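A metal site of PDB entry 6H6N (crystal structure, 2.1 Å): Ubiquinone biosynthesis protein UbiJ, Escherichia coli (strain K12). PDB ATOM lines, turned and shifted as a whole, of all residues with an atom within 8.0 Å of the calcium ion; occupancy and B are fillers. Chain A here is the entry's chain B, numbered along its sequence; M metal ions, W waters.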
ATOM      1  N   PHE A  29      22.719 -21.688 -12.873  1.00  0.00           N
ATOM      2  CA  PHE A  29      22.400 -20.284 -12.674  1.00  0.00           C
ATOM      3  C   PHE A  29      22.850 -19.355 -13.807  1.00  0.00           C
ATOM      4  O   PHE A  29      22.091 -18.495 -14.190  1.00  0.00           O
ATOM      5  CB  PHE A  29      22.969 -19.807 -11.308  1.00  0.00           C
ATOM      6  CG  PHE A  29      22.595 -18.402 -10.923  1.00  0.00           C
ATOM      7  CD1 PHE A  29      21.266 -18.024 -10.793  1.00  0.00           C
ATOM      8  CD2 PHE A  29      23.586 -17.480 -10.584  1.00  0.00           C
ATOM      9  CE1 PHE A  29      20.931 -16.730 -10.416  1.00  0.00           C
ATOM     10  CE2 PHE A  29      23.245 -16.192 -10.196  1.00  0.00           C
ATOM     11  CZ  PHE A  29      21.919 -15.806 -10.124  1.00  0.00           C
ATOM     12  N   ARG A  93      25.577 -10.574  -6.548  1.00  0.00           N
ATOM     13  CA  ARG A  93      24.530 -10.676  -7.570  1.00  0.00           C
ATOM     14  C   ARG A  93      23.986  -9.253  -7.856  1.00  0.00           C
ATOM     15  O   ARG A  93      22.941  -9.095  -8.500  1.00  0.00           O
ATOM     16  CB  ARG A  93      23.391 -11.602  -7.117  1.00  0.00           C
ATOM     17  CG  ARG A  93      23.747 -13.088  -7.080  1.00  0.00           C
ATOM     18  CD  ARG A  93      22.632 -13.880  -6.422  1.00  0.00           C
ATOM     19  NE  ARG A  93      22.735 -13.900  -4.962  1.00  0.00           N
ATOM     20  CZ  ARG A  93      21.705 -14.062  -4.132  1.00  0.00           C
ATOM     21  NH1 ARG A  93      20.474 -14.168  -4.603  1.00  0.00           N
ATOM     22  NH2 ARG A  93      21.902 -14.102  -2.826  1.00  0.00           N
ATOM     23  N   ASP A  94      24.702  -8.214  -7.369  1.00  0.00           N
ATOM     24  CA  ASP A  94      24.327  -6.822  -7.558  1.00  0.00           C
ATOM     25  C   ASP A  94      25.527  -5.971  -7.959  1.00  0.00           C
ATOM     26  O   ASP A  94      26.397  -5.673  -7.133  1.00  0.00           O
ATOM     27  CB  ASP A  94      23.617  -6.266  -6.319  1.00  0.00           C
ATOM     28  CG  ASP A  94      22.998  -4.865  -6.444  1.00  0.00           C
ATOM     29  OD1 ASP A  94      22.853  -4.382  -7.599  1.00  0.00           O
ATOM     30  OD2 ASP A  94      22.600  -4.302  -5.402  1.00  0.00           O
ATOM     31  N   ARG A  95      25.546  -5.577  -9.244  1.00  0.00           N
ATOM     32  CA  ARG A  95      26.567  -4.747  -9.876  1.00  0.00           C
ATOM     33  C   ARG A  95      26.756  -3.373  -9.270  1.00  0.00           C
ATOM     34  O   ARG A  95      27.872  -2.854  -9.279  1.00  0.00           O
ATOM     35  CB  ARG A  95      26.297  -4.588 -11.392  1.00  0.00           C
ATOM     36  CG  ARG A  95      27.594  -4.707 -12.180  1.00  0.00           C
ATOM     37  CD  ARG A  95      27.763  -3.807 -13.374  1.00  0.00           C
ATOM     38  NE  ARG A  95      29.066  -4.085 -13.988  1.00  0.00           N
ATOM     39  CZ  ARG A  95      29.532  -3.553 -15.114  1.00  0.00           C
ATOM     40  NH1 ARG A  95      30.715  -3.900 -15.583  1.00  0.00           N
ATOM     41  NH2 ARG A  95      28.804  -2.658 -15.778  1.00  0.00           N
ATOM     42  N   VAL A 120      30.065 -10.239 -11.598  1.00  0.00           N
ATOM     43  CA  VAL A 120      28.974  -9.639 -10.818  1.00  0.00           C
ATOM     44  C   VAL A 120      27.884  -9.103 -11.808  1.00  0.00           C
ATOM     45  O   VAL A 120      26.721  -9.346 -11.587  1.00  0.00           O
ATOM     46  CB  VAL A 120      29.503  -8.551  -9.844  1.00  0.00           C
ATOM     47  CG1 VAL A 120      28.381  -7.690  -9.281  1.00  0.00           C
ATOM     48  CG2 VAL A 120      30.274  -9.185  -8.694  1.00  0.00           C
ATOM     49  N   ALA A 121      28.280  -8.438 -12.905  1.00  0.00           N
ATOM     50  CA  ALA A 121      27.325  -7.950 -13.928  1.00  0.00           C
ATOM     51  C   ALA A 121      26.550  -9.153 -14.549  1.00  0.00           C
ATOM     52  O   ALA A 121      25.362  -9.028 -14.760  1.00  0.00           O
ATOM     53  CB  ALA A 121      28.079  -7.193 -15.021  1.00  0.00           C
ATOM     54  N   LEU A 122      27.236 -10.298 -14.794  1.00  0.00           N
ATOM     55  CA  LEU A 122      26.632 -11.532 -15.335  1.00  0.00           C
ATOM     56  C   LEU A 122      25.599 -12.128 -14.338  1.00  0.00           C
ATOM     57  O   LEU A 122      24.468 -12.407 -14.730  1.00  0.00           O
ATOM     58  CB  LEU A 122      27.712 -12.570 -15.699  1.00  0.00           C
ATOM     59  CG  LEU A 122      27.216 -14.011 -16.056  1.00  0.00           C
ATOM     60  CD1 LEU A 122      26.270 -14.017 -17.265  1.00  0.00           C
ATOM     61  CD2 LEU A 122      28.363 -14.976 -16.257  1.00  0.00           C
ATOM     62  N   ALA A 123      26.006 -12.301 -13.065  1.00  0.00           N
ATOM     63  CA  ALA A 123      25.169 -12.839 -11.979  1.00  0.00           C
ATOM     64  C   ALA A 123      23.955 -11.982 -11.767  1.00  0.00           C
ATOM     65  O   ALA A 123      22.886 -12.534 -11.528  1.00  0.00           O
ATOM     66  CB  ALA A 123      25.962 -12.972 -10.692  1.00  0.00           C
ATOM     67  N   ASP A 124      24.106 -10.645 -11.890  1.00  0.00           N
ATOM     68  CA  ASP A 124      23.006  -9.691 -11.765  1.00  0.00           C
ATOM     69  C   ASP A 124      22.005  -9.859 -12.922  1.00  0.00           C
ATOM     70  O   ASP A 124      20.814  -9.898 -12.692  1.00  0.00           O
ATOM     71  CB  ASP A 124      23.536  -8.243 -11.695  1.00  0.00           C
ATOM     72  CG  ASP A 124      22.529  -7.220 -11.202  1.00  0.00           C
ATOM     73  OD1 ASP A 124      21.381  -7.601 -10.883  1.00  0.00           O
ATOM     74  OD2 ASP A 124      22.902  -6.048 -11.084  1.00  0.00           O
ATOM     75  N   LEU A 125      22.512 -10.014 -14.144  1.00  0.00           N
ATOM     76  CA  LEU A 125      21.634 -10.250 -15.306  1.00  0.00           C
ATOM     77  C   LEU A 125      21.006 -11.667 -15.276  1.00  0.00           C
ATOM     78  O   LEU A 125      19.963 -11.876 -15.868  1.00  0.00           O
ATOM     79  CB  LEU A 125      22.404 -10.054 -16.608  1.00  0.00           C
ATOM     80  CG  LEU A 125      22.761  -8.618 -16.942  1.00  0.00           C
ATOM     81  CD1 LEU A 125      23.828  -8.561 -18.007  1.00  0.00           C
ATOM     82  CD2 LEU A 125      21.513  -7.788 -17.296  1.00  0.00           C
ATOM     83  N   ALA A 126      21.642 -12.621 -14.562  1.00  0.00           N
ATOM     84  CA  ALA A 126      21.126 -13.996 -14.440  1.00  0.00           C
ATOM     85  C   ALA A 126      19.889 -14.071 -13.554  1.00  0.00           C
ATOM     86  O   ALA A 126      19.118 -15.018 -13.652  1.00  0.00           O
ATOM     87  CB  ALA A 126      22.208 -14.906 -13.893  1.00  0.00           C
ATOM     88  N   GLU A 127      19.681 -13.077 -12.684  1.00  0.00           N
ATOM     89  CA  GLU A 127      18.587 -13.182 -11.727  1.00  0.00           C
ATOM     90  C   GLU A 127      17.666 -11.993 -11.695  1.00  0.00           C
ATOM     91  O   GLU A 127      18.120 -10.845 -11.731  1.00  0.00           O
ATOM     92  CB  GLU A 127      19.232 -13.447 -10.356  1.00  0.00           C
ATOM     93  CG  GLU A 127      18.391 -13.266  -9.107  1.00  0.00           C
ATOM     94  CD  GLU A 127      19.276 -13.209  -7.880  1.00  0.00           C
ATOM     95  OE1 GLU A 127      19.363 -14.227  -7.167  1.00  0.00           O
ATOM     96  OE2 GLU A 127      19.957 -12.183  -7.686  1.00  0.00           O
ATOM     97  N   PHE A 128      16.356 -12.276 -11.588  1.00  0.00           N
ATOM     98  CA  PHE A 128      15.293 -11.281 -11.437  1.00  0.00           C
ATOM     99  C   PHE A 128      15.349 -10.763  -9.992  1.00  0.00           C
ATOM    100  O   PHE A 128      15.509 -11.557  -9.086  1.00  0.00           O
ATOM    101  CB  PHE A 128      13.920 -11.925 -11.690  1.00  0.00           C
ATOM    102  CG  PHE A 128      13.500 -12.044 -13.128  1.00  0.00           C
ATOM    103  CD1 PHE A 128      13.005 -10.944 -13.822  1.00  0.00           C
ATOM    104  CD2 PHE A 128      13.593 -13.269 -13.800  1.00  0.00           C
ATOM    105  CE1 PHE A 128      12.598 -11.061 -15.159  1.00  0.00           C
ATOM    106  CE2 PHE A 128      13.185 -13.386 -15.138  1.00  0.00           C
ATOM    107  CZ  PHE A 128      12.693 -12.280 -15.808  1.00  0.00           C
ATOM    108  N   ASP A 129      15.264  -9.455  -9.801  1.00  0.00           N
ATOM    109  CA  ASP A 129      15.304  -8.843  -8.462  1.00  0.00           C
ATOM    110  C   ASP A 129      13.921  -8.896  -7.810  1.00  0.00           C
ATOM    111  O   ASP A 129      12.904  -8.773  -8.491  1.00  0.00           O
ATOM    112  CB  ASP A 129      15.814  -7.387  -8.526  1.00  0.00           C
ATOM    113  CG  ASP A 129      17.267  -7.249  -8.934  1.00  0.00           C
ATOM    114  OD1 ASP A 129      17.675  -7.889  -9.929  1.00  0.00           O
ATOM    115  OD2 ASP A 129      17.992  -6.450  -8.295  1.00  0.00           O
HETATM  116 CA    CA M   1      19.534  -9.092 -11.014  1.00  0.00          CA
HETATM  117  O   HOH W   1      20.321  -9.951  -9.207  1.00  0.00           O
HETATM  118  O   HOH W   2      18.723  -8.244 -13.217  1.00  0.00           O
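Three residues have an atom within 4 Å of the calcium ion: Asp 124, Glu 127 and Asp 129.
The nearest printed residue that does not touch the calcium ion is Arg 93 (4.2 Å).
OD2 of Asp 124 is in hydrogen-bond range of N of Arg 95, at 3.3 Å.
The guanidinium group (NH1) of Arg 93 lies within salt-bridge range of the side-chain carboxylate (OE1) of Glu 127 (2.8 Å).
Water W1 is bound to the calcium ion, at 2.1 Å.
The backbone carbonyl oxygen (O) of Asp 124 binds the calcium ion (2.3 Å).
The calcium ion is bound by O of Glu 127 (2.4 Å).
OD1 of Asp 124 binds the calcium ion (2.4 Å).
The side-chain carboxylate (OD1) of Asp 129 binds the calcium ion, 2.5 Å away.
The calcium ion is bound by water W2.
Water W1 bridges the side-chain carboxylate (OE2) of Glu 127 (2.7 Å) and the backbone carbonyl oxygen (O) of Arg 93 (2.8 Å).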
